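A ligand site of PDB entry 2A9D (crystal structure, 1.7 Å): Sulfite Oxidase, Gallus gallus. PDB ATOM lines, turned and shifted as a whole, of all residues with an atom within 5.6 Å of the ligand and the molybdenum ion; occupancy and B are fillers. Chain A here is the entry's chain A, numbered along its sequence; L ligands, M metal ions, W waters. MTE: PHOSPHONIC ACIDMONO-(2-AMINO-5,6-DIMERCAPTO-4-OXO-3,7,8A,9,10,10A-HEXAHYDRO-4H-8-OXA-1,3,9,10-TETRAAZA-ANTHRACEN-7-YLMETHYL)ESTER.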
ATOM      1  N   PHE A  41      -8.865   0.426   8.194  1.00  0.00           N
ATOM      2  CA  PHE A  41      -8.524   1.848   7.917  1.00  0.00           C
ATOM      3  C   PHE A  41      -8.435   2.018   6.391  1.00  0.00           C
ATOM      4  O   PHE A  41      -7.800   1.202   5.695  1.00  0.00           O
ATOM      5  CB  PHE A  41      -7.215   2.186   8.651  1.00  0.00           C
ATOM      6  CG  PHE A  41      -6.938   3.662   8.817  1.00  0.00           C
ATOM      7  CD1 PHE A  41      -6.550   4.444   7.740  1.00  0.00           C
ATOM      8  CD2 PHE A  41      -7.022   4.265  10.067  1.00  0.00           C
ATOM      9  CE1 PHE A  41      -6.285   5.763   7.895  1.00  0.00           C
ATOM     10  CE2 PHE A  41      -6.788   5.611  10.221  1.00  0.00           C
ATOM     11  CZ  PHE A  41      -6.411   6.352   9.124  1.00  0.00           C
ATOM     12  N   PHE A  42      -9.089   3.034   5.844  1.00  0.00           N
ATOM     13  CA  PHE A  42      -9.096   3.190   4.385  1.00  0.00           C
ATOM     14  C   PHE A  42      -7.669   3.329   3.873  1.00  0.00           C
ATOM     15  O   PHE A  42      -6.773   3.860   4.560  1.00  0.00           O
ATOM     16  CB  PHE A  42      -9.965   4.366   3.934  1.00  0.00           C
ATOM     17  CG  PHE A  42      -9.240   5.681   3.924  1.00  0.00           C
ATOM     18  CD1 PHE A  42      -9.101   6.413   5.098  1.00  0.00           C
ATOM     19  CD2 PHE A  42      -8.777   6.238   2.726  1.00  0.00           C
ATOM     20  CE1 PHE A  42      -8.460   7.662   5.095  1.00  0.00           C
ATOM     21  CE2 PHE A  42      -8.098   7.448   2.718  1.00  0.00           C
ATOM     22  CZ  PHE A  42      -7.945   8.179   3.912  1.00  0.00           C
ATOM     23  N   THR A  43      -7.465   2.900   2.633  1.00  0.00           N
ATOM     24  CA  THR A  43      -6.147   2.895   2.040  1.00  0.00           C
ATOM     25  C   THR A  43      -6.138   3.641   0.713  1.00  0.00           C
ATOM     26  O   THR A  43      -6.986   3.378  -0.148  1.00  0.00           O
ATOM     27  CB  THR A  43      -5.666   1.438   1.844  1.00  0.00           C
ATOM     28  OG1 THR A  43      -5.559   0.809   3.110  1.00  0.00           O
ATOM     29  CG2 THR A  43      -4.298   1.417   1.155  1.00  0.00           C
ATOM     30  N   ARG A  44      -5.249   4.629   0.589  1.00  0.00           N
ATOM     31  CA  ARG A  44      -5.127   5.387  -0.667  1.00  0.00           C
ATOM     32  C   ARG A  44      -3.670   5.405  -1.082  1.00  0.00           C
ATOM     33  O   ARG A  44      -2.836   6.040  -0.435  1.00  0.00           O
ATOM     34  CB  ARG A  44      -5.713   6.784  -0.525  1.00  0.00           C
ATOM     35  CG  ARG A  44      -6.130   7.417  -1.847  1.00  0.00           C
ATOM     36  CD  ARG A  44      -4.988   7.974  -2.620  1.00  0.00           C
ATOM     37  NE  ARG A  44      -5.386   8.586  -3.891  1.00  0.00           N
ATOM     38  CZ  ARG A  44      -5.250   8.022  -5.086  1.00  0.00           C
ATOM     39  NH1 ARG A  44      -4.782   6.798  -5.200  1.00  0.00           N
ATOM     40  NH2 ARG A  44      -5.605   8.696  -6.174  1.00  0.00           N
ATOM     41  N   ASN A  45      -3.368   4.623  -2.125  1.00  0.00           N
ATOM     42  CA  ASN A  45      -2.027   4.529  -2.705  1.00  0.00           C
ATOM     43  C   ASN A  45      -2.048   4.996  -4.161  1.00  0.00           C
ATOM     44  O   ASN A  45      -2.840   4.509  -4.954  1.00  0.00           O
ATOM     45  CB  ASN A  45      -1.502   3.078  -2.701  1.00  0.00           C
ATOM     46  CG  ASN A  45      -1.464   2.409  -1.333  1.00  0.00           C
ATOM     47  OD1 ASN A  45      -1.360   3.061  -0.274  1.00  0.00           O
ATOM     48  ND2 ASN A  45      -1.516   1.072  -1.341  1.00  0.00           N
ATOM     49  N   HIS A  46      -1.210   5.969  -4.510  1.00  0.00           N
ATOM     50  CA  HIS A  46      -1.089   6.439  -5.876  1.00  0.00           C
ATOM     51  C   HIS A  46      -0.131   5.573  -6.684  1.00  0.00           C
ATOM     52  O   HIS A  46      -0.195   5.522  -7.918  1.00  0.00           O
ATOM     53  CB  HIS A  46      -0.507   7.847  -5.921  1.00  0.00           C
ATOM     54  CG  HIS A  46      -1.450   8.919  -5.443  1.00  0.00           C
ATOM     55  ND1 HIS A  46      -1.618   9.215  -4.111  1.00  0.00           N
ATOM     56  CD2 HIS A  46      -2.268   9.750  -6.125  1.00  0.00           C
ATOM     57  CE1 HIS A  46      -2.465  10.234  -4.001  1.00  0.00           C
ATOM     58  NE2 HIS A  46      -2.896  10.549  -5.210  1.00  0.00           N
ATOM     59  N   LEU A  47       0.759   4.886  -5.965  1.00  0.00           N
ATOM     60  CA  LEU A  47       1.846   4.142  -6.616  1.00  0.00           C
ATOM     61  C   LEU A  47       2.054   2.790  -5.957  1.00  0.00           C
ATOM     62  O   LEU A  47       1.395   2.465  -4.977  1.00  0.00           O
ATOM     63  CB  LEU A  47       3.126   4.987  -6.483  1.00  0.00           C
ATOM     64  CG  LEU A  47       3.091   6.355  -7.179  1.00  0.00           C
ATOM     65  CD1 LEU A  47       4.175   7.277  -6.659  1.00  0.00           C
ATOM     66  CD2 LEU A  47       3.194   6.188  -8.689  1.00  0.00           C
ATOM     67  N   LEU A  89      -7.798  10.825   9.468  1.00  0.00           N
ATOM     68  CA  LEU A  89      -7.390  11.176   8.118  1.00  0.00           C
ATOM     69  C   LEU A  89      -8.595  11.067   7.192  1.00  0.00           C
ATOM     70  O   LEU A  89      -9.303  10.036   7.205  1.00  0.00           O
ATOM     71  CB  LEU A  89      -6.273  10.258   7.626  1.00  0.00           C
ATOM     72  CG  LEU A  89      -4.953  10.285   8.391  1.00  0.00           C
ATOM     73  CD1 LEU A  89      -3.958   9.349   7.729  1.00  0.00           C
ATOM     74  CD2 LEU A  89      -4.364  11.667   8.451  1.00  0.00           C
ATOM     75  N   GLN A  90      -8.906  12.152   6.501  1.00  0.00           N
ATOM     76  CA  GLN A  90      -9.944  12.156   5.484  1.00  0.00           C
ATOM     77  C   GLN A  90      -9.344  12.493   4.151  1.00  0.00           C
ATOM     78  O   GLN A  90      -8.605  13.487   4.024  1.00  0.00           O
ATOM     79  CB  GLN A  90     -11.030  13.189   5.775  1.00  0.00           C
ATOM     80  CG  GLN A  90     -12.177  13.106   4.804  1.00  0.00           C
ATOM     81  CD  GLN A  90     -13.219  14.136   4.978  1.00  0.00           C
ATOM     82  OE1 GLN A  90     -13.102  15.079   5.824  1.00  0.00           O
ATOM     83  NE2 GLN A  90     -14.257  14.022   4.170  1.00  0.00           N
ATOM     84  N   CYS A  91      -9.640  11.688   3.144  1.00  0.00           N
ATOM     85  CA  CYS A  91      -9.196  11.952   1.803  1.00  0.00           C
ATOM     86  C   CYS A  91     -10.012  13.089   1.192  1.00  0.00           C
ATOM     87  O   CYS A  91     -11.245  13.230   1.407  1.00  0.00           O
ATOM     88  CB  CYS A  91      -9.386  10.725   0.923  1.00  0.00           C
ATOM     89  SG  CYS A  91      -8.662  10.712  -0.718  1.00  0.00           S
ATOM     90  N   ALA A  92      -9.296  13.896   0.384  1.00  0.00           N
ATOM     91  CA  ALA A  92      -9.907  14.950  -0.431  1.00  0.00           C
ATOM     92  C   ALA A  92     -11.095  14.389  -1.214  1.00  0.00           C
ATOM     93  O   ALA A  92     -12.058  15.128  -1.492  1.00  0.00           O
ATOM     94  CB  ALA A  92      -8.885  15.547  -1.423  1.00  0.00           C
ATOM     95  N   GLY A  93     -10.992  13.141  -1.641  1.00  0.00           N
ATOM     96  CA  GLY A  93     -12.068  12.531  -2.431  1.00  0.00           C
ATOM     97  C   GLY A  93     -13.184  11.838  -1.689  1.00  0.00           C
ATOM     98  O   GLY A  93     -14.070  11.225  -2.312  1.00  0.00           O
ATOM     99  N   TRP A 120      -1.924   7.642  16.554  1.00  0.00           N
ATOM    100  CA  TRP A 120      -0.597   7.575  15.937  1.00  0.00           C
ATOM    101  C   TRP A 120       0.481   7.834  16.975  1.00  0.00           C
ATOM    102  O   TRP A 120       0.310   8.663  17.879  1.00  0.00           O
ATOM    103  CB  TRP A 120      -0.487   8.619  14.820  1.00  0.00           C
ATOM    104  CG  TRP A 120      -1.594   8.571  13.839  1.00  0.00           C
ATOM    105  CD1 TRP A 120      -2.753   9.299  13.888  1.00  0.00           C
ATOM    106  CD2 TRP A 120      -1.709   7.717  12.676  1.00  0.00           C
ATOM    107  NE1 TRP A 120      -3.574   8.957  12.828  1.00  0.00           N
ATOM    108  CE2 TRP A 120      -2.939   8.024  12.047  1.00  0.00           C
ATOM    109  CE3 TRP A 120      -0.866   6.776  12.071  1.00  0.00           C
ATOM    110  CZ2 TRP A 120      -3.371   7.371  10.899  1.00  0.00           C
ATOM    111  CZ3 TRP A 120      -1.293   6.145  10.921  1.00  0.00           C
ATOM    112  CH2 TRP A 120      -2.530   6.445  10.337  1.00  0.00           C
ATOM    113  N   GLY A 148       8.057  10.734  -0.542  1.00  0.00           N
ATOM    114  CA  GLY A 148       7.888   9.323  -0.196  1.00  0.00           C
ATOM    115  C   GLY A 148       8.871   8.449  -0.975  1.00  0.00           C
ATOM    116  O   GLY A 148       9.525   8.921  -1.903  1.00  0.00           O
ATOM    117  N   LEU A 149       8.975   7.180  -0.573  1.00  0.00           N
ATOM    118  CA  LEU A 149       9.831   6.203  -1.254  1.00  0.00           C
ATOM    119  C   LEU A 149       9.144   5.630  -2.507  1.00  0.00           C
ATOM    120  O   LEU A 149       9.788   4.947  -3.316  1.00  0.00           O
ATOM    121  CB  LEU A 149      10.191   5.067  -0.310  1.00  0.00           C
ATOM    122  CG  LEU A 149      11.225   5.324   0.774  1.00  0.00           C
ATOM    123  CD1 LEU A 149      11.138   4.244   1.842  1.00  0.00           C
ATOM    124  CD2 LEU A 149      12.646   5.438   0.195  1.00  0.00           C
ATOM    125  N   ASP A 150       7.843   5.869  -2.639  1.00  0.00           N
ATOM    126  CA  ASP A 150       7.073   5.431  -3.810  1.00  0.00           C
ATOM    127  C   ASP A 150       7.287   6.409  -4.980  1.00  0.00           C
ATOM    128  O   ASP A 150       7.267   7.622  -4.778  1.00  0.00           O
ATOM    129  CB  ASP A 150       5.570   5.231  -3.489  1.00  0.00           C
ATOM    130  CG  ASP A 150       4.886   6.455  -2.861  1.00  0.00           C
ATOM    131  OD1 ASP A 150       5.524   7.196  -2.070  1.00  0.00           O
ATOM    132  OD2 ASP A 150       3.666   6.629  -3.119  1.00  0.00           O
ATOM    133  N   TYR A 158       6.118  10.428  -4.650  1.00  0.00           N
ATOM    134  CA  TYR A 158       4.955  11.125  -4.123  1.00  0.00           C
ATOM    135  C   TYR A 158       5.500  12.181  -3.163  1.00  0.00           C
ATOM    136  O   TYR A 158       6.436  11.941  -2.422  1.00  0.00           O
ATOM    137  CB  TYR A 158       3.977  10.196  -3.382  1.00  0.00           C
ATOM    138  CG  TYR A 158       2.753  10.957  -2.918  1.00  0.00           C
ATOM    139  CD1 TYR A 158       1.696  11.201  -3.799  1.00  0.00           C
ATOM    140  CD2 TYR A 158       2.665  11.512  -1.623  1.00  0.00           C
ATOM    141  CE1 TYR A 158       0.617  11.923  -3.420  1.00  0.00           C
ATOM    142  CE2 TYR A 158       1.562  12.214  -1.229  1.00  0.00           C
ATOM    143  CZ  TYR A 158       0.546  12.453  -2.143  1.00  0.00           C
ATOM    144  OH  TYR A 158      -0.552  13.196  -1.816  1.00  0.00           O
ATOM    145  N   ASP A 188       0.750  -0.876   3.972  1.00  0.00           N
ATOM    146  CA  ASP A 188      -0.171   0.003   3.231  1.00  0.00           C
ATOM    147  C   ASP A 188      -0.283   1.411   3.834  1.00  0.00           C
ATOM    148  O   ASP A 188      -0.738   2.326   3.156  1.00  0.00           O
ATOM    149  CB  ASP A 188      -1.580  -0.603   3.079  1.00  0.00           C
ATOM    150  CG  ASP A 188      -1.722  -1.520   1.871  1.00  0.00           C
ATOM    151  OD1 ASP A 188      -1.018  -1.309   0.854  1.00  0.00           O
ATOM    152  OD2 ASP A 188      -2.552  -2.464   1.911  1.00  0.00           O
ATOM    153  N   HIS A 189       0.037   1.565   5.113  1.00  0.00           N
ATOM    154  CA  HIS A 189      -0.078   2.865   5.803  1.00  0.00           C
ATOM    155  C   HIS A 189       1.249   3.569   6.059  1.00  0.00           C
ATOM    156  O   HIS A 189       1.314   4.520   6.862  1.00  0.00           O
ATOM    157  CB  HIS A 189      -0.971   2.727   7.048  1.00  0.00           C
ATOM    158  CG  HIS A 189      -2.344   2.216   6.726  1.00  0.00           C
ATOM    159  ND1 HIS A 189      -3.260   2.983   6.030  1.00  0.00           N
ATOM    160  CD2 HIS A 189      -2.918   0.994   6.889  1.00  0.00           C
ATOM    161  CE1 HIS A 189      -4.362   2.266   5.844  1.00  0.00           C
ATOM    162  NE2 HIS A 189      -4.152   1.047   6.304  1.00  0.00           N
ATOM    163  N   ARG A 194       5.651   7.474   8.437  1.00  0.00           N
ATOM    164  CA  ARG A 194       4.837   8.383   7.642  1.00  0.00           C
ATOM    165  C   ARG A 194       4.727   9.709   8.374  1.00  0.00           C
ATOM    166  O   ARG A 194       4.911   9.774   9.589  1.00  0.00           O
ATOM    167  CB  ARG A 194       3.424   7.847   7.445  1.00  0.00           C
ATOM    168  CG  ARG A 194       2.495   8.070   8.631  1.00  0.00           C
ATOM    169  CD  ARG A 194       1.095   7.646   8.352  1.00  0.00           C
ATOM    170  NE  ARG A 194       0.443   8.418   7.285  1.00  0.00           N
ATOM    171  CZ  ARG A 194      -0.606   7.993   6.602  1.00  0.00           C
ATOM    172  NH1 ARG A 194      -1.212   6.845   6.927  1.00  0.00           N
ATOM    173  NH2 ARG A 194      -1.099   8.717   5.624  1.00  0.00           N
ATOM    174  N   VAL A 201      -6.017  17.558   5.096  1.00  0.00           N
ATOM    175  CA  VAL A 201      -6.367  16.554   4.101  1.00  0.00           C
ATOM    176  C   VAL A 201      -5.356  15.420   4.043  1.00  0.00           C
ATOM    177  O   VAL A 201      -4.150  15.629   4.178  1.00  0.00           O
ATOM    178  CB  VAL A 201      -6.620  17.209   2.735  1.00  0.00           C
ATOM    179  CG1 VAL A 201      -5.339  17.764   2.159  1.00  0.00           C
ATOM    180  CG2 VAL A 201      -7.333  16.260   1.735  1.00  0.00           C
ATOM    181  N   GLY A 202      -5.848  14.204   3.804  1.00  0.00           N
ATOM    182  CA  GLY A 202      -4.975  13.046   3.887  1.00  0.00           C
ATOM    183  C   GLY A 202      -3.741  13.130   2.988  1.00  0.00           C
ATOM    184  O   GLY A 202      -2.676  12.575   3.310  1.00  0.00           O
ATOM    185  N   ALA A 203      -3.905  13.786   1.848  1.00  0.00           N
ATOM    186  CA  ALA A 203      -2.865  13.908   0.818  1.00  0.00           C
ATOM    187  C   ALA A 203      -1.523  14.410   1.338  1.00  0.00           C
ATOM    188  O   ALA A 203      -0.475  14.033   0.825  1.00  0.00           O
ATOM    189  CB  ALA A 203      -3.329  14.797  -0.341  1.00  0.00           C
ATOM    190  N   ARG A 204      -1.551  15.187   2.418  1.00  0.00           N
ATOM    191  CA  ARG A 204      -0.321  15.763   2.926  1.00  0.00           C
ATOM    192  C   ARG A 204       0.422  14.868   3.912  1.00  0.00           C
ATOM    193  O   ARG A 204       1.573  15.156   4.230  1.00  0.00           O
ATOM    194  CB  ARG A 204      -0.588  17.121   3.551  1.00  0.00           C
ATOM    195  CG  ARG A 204      -1.388  18.081   2.714  1.00  0.00           C
ATOM    196  CD  ARG A 204      -0.844  18.309   1.284  1.00  0.00           C
ATOM    197  NE  ARG A 204      -1.877  19.063   0.550  1.00  0.00           N
ATOM    198  CZ  ARG A 204      -2.088  19.044  -0.763  1.00  0.00           C
ATOM    199  NH1 ARG A 204      -1.319  18.363  -1.596  1.00  0.00           N
ATOM    200  NH2 ARG A 204      -3.107  19.737  -1.261  1.00  0.00           N
ATOM    201  N   SER A 205      -0.224  13.780   4.329  1.00  0.00           N
ATOM    202  CA  SER A 205       0.344  12.840   5.302  1.00  0.00           C
ATOM    203  C   SER A 205       1.146  11.776   4.555  1.00  0.00           C
ATOM    204  O   SER A 205       0.744  10.606   4.459  1.00  0.00           O
ATOM    205  CB  SER A 205      -0.764  12.226   6.167  1.00  0.00           C
ATOM    206  OG  SER A 205      -1.274  13.168   7.122  1.00  0.00           O
ATOM    207  N   VAL A 206       2.300  12.205   4.047  1.00  0.00           N
ATOM    208  CA  VAL A 206       3.183  11.384   3.221  1.00  0.00           C
ATOM    209  C   VAL A 206       3.679  10.100   3.905  1.00  0.00           C
ATOM    210  O   VAL A 206       4.305  10.131   4.940  1.00  0.00           O
ATOM    211  CB  VAL A 206       4.375  12.193   2.702  1.00  0.00           C
ATOM    212  CG1 VAL A 206       5.316  11.295   1.906  1.00  0.00           C
ATOM    213  CG2 VAL A 206       3.872  13.382   1.852  1.00  0.00           C
ATOM    214  N   LYS A 207       3.393   8.992   3.245  1.00  0.00           N
ATOM    215  CA  LYS A 207       3.756   7.668   3.700  1.00  0.00           C
ATOM    216  C   LYS A 207       5.121   7.257   3.126  1.00  0.00           C
ATOM    217  O   LYS A 207       5.560   7.785   2.099  1.00  0.00           O
ATOM    218  CB  LYS A 207       2.692   6.682   3.232  1.00  0.00           C
ATOM    219  CG  LYS A 207       1.290   6.849   3.863  1.00  0.00           C
ATOM    220  CD  LYS A 207       0.329   5.743   3.461  1.00  0.00           C
ATOM    221  CE  LYS A 207      -0.295   5.935   2.061  1.00  0.00           C
ATOM    222  NZ  LYS A 207      -1.285   4.848   1.755  1.00  0.00           N
ATOM    223  N   TRP A 208       5.727   6.271   3.779  1.00  0.00           N
ATOM    224  CA  TRP A 208       7.037   5.746   3.358  1.00  0.00           C
ATOM    225  C   TRP A 208       8.017   6.896   3.194  1.00  0.00           C
ATOM    226  O   TRP A 208       8.731   6.985   2.192  1.00  0.00           O
ATOM    227  CB  TRP A 208       6.884   4.972   2.047  1.00  0.00           C
ATOM    228  CG  TRP A 208       5.764   3.992   2.064  1.00  0.00           C
ATOM    229  CD1 TRP A 208       5.727   2.814   2.751  1.00  0.00           C
ATOM    230  CD2 TRP A 208       4.526   4.087   1.358  1.00  0.00           C
ATOM    231  NE1 TRP A 208       4.528   2.195   2.554  1.00  0.00           N
ATOM    232  CE2 TRP A 208       3.774   2.950   1.693  1.00  0.00           C
ATOM    233  CE3 TRP A 208       3.997   5.016   0.458  1.00  0.00           C
ATOM    234  CZ2 TRP A 208       2.520   2.710   1.140  1.00  0.00           C
ATOM    235  CZ3 TRP A 208       2.759   4.765  -0.072  1.00  0.00           C
ATOM    236  CH2 TRP A 208       2.010   3.666   0.302  1.00  0.00           C
ATOM    237  N   TYR A 228      -5.562  18.204  -6.042  1.00  0.00           N
ATOM    238  CA  TYR A 228      -6.112  18.535  -4.732  1.00  0.00           C
ATOM    239  C   TYR A 228      -6.317  20.032  -4.464  1.00  0.00           C
ATOM    240  O   TYR A 228      -5.805  20.616  -3.512  1.00  0.00           O
ATOM    241  CB  TYR A 228      -5.223  17.894  -3.650  1.00  0.00           C
ATOM    242  CG  TYR A 228      -5.117  16.408  -3.812  1.00  0.00           C
ATOM    243  CD1 TYR A 228      -6.249  15.617  -3.806  1.00  0.00           C
ATOM    244  CD2 TYR A 228      -3.866  15.790  -4.017  1.00  0.00           C
ATOM    245  CE1 TYR A 228      -6.178  14.264  -3.942  1.00  0.00           C
ATOM    246  CE2 TYR A 228      -3.779  14.447  -4.193  1.00  0.00           C
ATOM    247  CZ  TYR A 228      -4.930  13.672  -4.132  1.00  0.00           C
ATOM    248  OH  TYR A 228      -4.848  12.304  -4.256  1.00  0.00           O
HETATM  249  N1  MTE L   1       1.915   9.147   0.659  1.00  0.00           N
HETATM  250  C2  MTE L   1       2.611   8.439  -0.244  1.00  0.00           C
HETATM  251  N2  MTE L   1       3.923   8.345  -0.191  1.00  0.00           N
HETATM  252  N3  MTE L   1       1.983   8.072  -1.401  1.00  0.00           N
HETATM  253  C4  MTE L   1       0.645   8.331  -1.642  1.00  0.00           C
HETATM  254  O4  MTE L   1       0.140   7.804  -2.676  1.00  0.00           O
HETATM  255  N5  MTE L   1      -1.479   9.137  -0.669  1.00  0.00           N
HETATM  256  C6  MTE L   1      -1.977  10.180   0.088  1.00  0.00           C
HETATM  257  C7  MTE L   1      -1.356  10.176   1.531  1.00  0.00           C
HETATM  258  N8  MTE L   1      -0.015   9.819   1.588  1.00  0.00           N
HETATM  259  C9  MTE L   1      -0.128   8.812  -0.556  1.00  0.00           C
HETATM  260  C10 MTE L   1       0.579   9.166   0.590  1.00  0.00           C
HETATM  261  C1' MTE L   1      -3.395  10.296   0.172  1.00  0.00           C
HETATM  262  S1' MTE L   1      -4.052  11.153  -1.193  1.00  0.00           S
HETATM  263  C2' MTE L   1      -4.088  10.065   1.306  1.00  0.00           C
HETATM  264  S2' MTE L   1      -5.839  10.297   1.301  1.00  0.00           S
HETATM  265  C3' MTE L   1      -3.452   9.370   2.474  1.00  0.00           C
HETATM  266  O3' MTE L   1      -2.058   9.135   2.280  1.00  0.00           O
HETATM  267  C4' MTE L   1      -4.087   8.067   2.802  1.00  0.00           C
HETATM  268  O4' MTE L   1      -3.493   7.438   3.963  1.00  0.00           O
HETATM  269  P   MTE L   1      -3.951   5.955   4.215  1.00  0.00           P
HETATM  270  O1P MTE L   1      -3.781   5.185   3.000  1.00  0.00           O
HETATM  271  O2P MTE L   1      -5.361   6.041   4.628  1.00  0.00           O
HETATM  272  O3P MTE L   1      -2.961   5.483   5.331  1.00  0.00           O
HETATM  273 MO    MO M   1      -6.357  11.603  -0.637  1.00  0.00          MO
HETATM  274  O   HOH W   1       1.586   4.849  -3.257  1.00  0.00           O
HETATM  275  O   HOH W   2      -6.324  13.318   0.000  1.00  0.00           O
HETATM  276  O   HOH W   3      -6.715  11.387  -2.779  1.00  0.00           O
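The side-chain sulfur (SG) of Cys 91 sits close to the backbone NH (N) of Gly 93 (3.5 Å).
OG1 of Thr 43 lies close to NE2 of His 189 (3.5 Å).
A ring nitrogen (NE2) of His 46 sits at hydrogen-bond distance from the guanidinium group of Arg 44, 3.4 Å away.
O of Ser 205 sits at hydrogen-bond distance from NH2 of Arg 194, at 2.9 Å.
The backbone NH of Gly 202 sits at hydrogen-bond distance from the backbone carbonyl oxygen of Gln 90 (2.9 Å).
O of Tyr 158 is in hydrogen-bond range of N of Gly 148 (2.8 Å).
N of Leu 149 sits at hydrogen-bond distance from O of Trp 208, at 2.8 Å.
O of Phe 41 lies within hydrogen-bond range of OG1 of Thr 43.
Water W3 lies within hydrogen-bond range of OH of Tyr 228 (2.6 Å) and NE of Arg 44 (3.3 Å).
Water W2 bridges N of Ala 92 (3.1 Å) and N of Ala 203 (3.1 Å).
Water W1 lies within hydrogen-bond range of the side-chain carboxylate of Asp 150 (2.7 Å), the backbone NH of Leu 47 (2.8 Å), the backbone NH of His 46 (3.3 Å) and an oxygen (O4) of the ligand (3.3 Å).
Phe 41 touches the ligand.
Thr 43 touches the ligand.
Asn 45 touches the ligand.
CG of Tyr 158 touches N3 of the ligand, at 3.3 Å.
O of Gly 202 touches C7 of the ligand (3.3 Å).
CA of Ala 203 touches S1' of the ligand, 3.6 Å away.
Val 206 touches the ligand (CA to N1, 3.6 Å).
CE3 of Trp 208 touches N2 of the ligand, at 3.4 Å.
Within 4 Å of the ligand: Phe 41, Phe 42, Thr 43, Arg 44, Asn 45, His 46, Cys 91, Asp 150, Tyr 158, His 189, Arg 194, Gly 202, Ala 203, Ser 205, Val 206, Lys 207, Trp 208 and Tyr 228.
Along chain A the residues within 4 Å of the ligand span positions 41 to 228.
Residues that only touch the molybdenum ion: Ala 92 (3.9 Å) and Tyr 228 (3.98 Å).
Along chain A the residues within 4 Å of the molybdenum ion span positions 91 to 228.
The nearest printed residue that does not touch the molybdenum ion is Ala 203 (4.1 Å).
The molybdenum ion is bound by water W2 (1.8 Å).
The molybdenum ion is bound by water W3 (2.2 Å).
S2' of the ligand is bound to the molybdenum ion.
S1' of the ligand binds the molybdenum ion.
SG of Cys 91 binds the molybdenum ion.
The molybdenum ion has five donor atoms within binding distance.
The backbone carbonyl oxygen of Phe 42 sits close to an oxygen (O2P) of the ligand, 2.6 Å away.
O3P of the ligand lies within hydrogen-bond range of ND1 of His 189, 2.6 Å away.
N of His 46 is in hydrogen-bond range of O4 of the ligand (2.9 Å).
A ring nitrogen (ND1) of His 46 is in hydrogen-bond range of an oxygen (O4) of the ligand.
OD1 of Asp 150 is in hydrogen-bond range of N2 of the ligand, at 2.7 Å.
The guanidinium group (NH1) of Arg 194 lies within salt-bridge range of an oxygen (O3P) of the ligand, at 2.7 Å.
The backbone NH (N) of Lys 207 sits at hydrogen-bond distance from a nitrogen (N1) of the ligand.
The backbone carbonyl oxygen of Lys 207 is in hydrogen-bond range of a nitrogen (N2) of the ligand (2.9 Å).
The side-chain amino group (NZ) of Lys 207 lies within salt-bridge range of an oxygen (O1P) of the ligand (2.8 Å).
N of Arg 44 is in hydrogen-bond range of O1P of the ligand (2.9 Å).
O of Arg 44 lies within hydrogen-bond range of N5 of the ligand (3.4 Å).
A nitrogen (N8) of the ligand is in hydrogen-bond range of the backbone carbonyl oxygen of Ser 205 (3.1 Å).
OH of Tyr 228 sits close to S1' of the ligand (3.4 Å).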
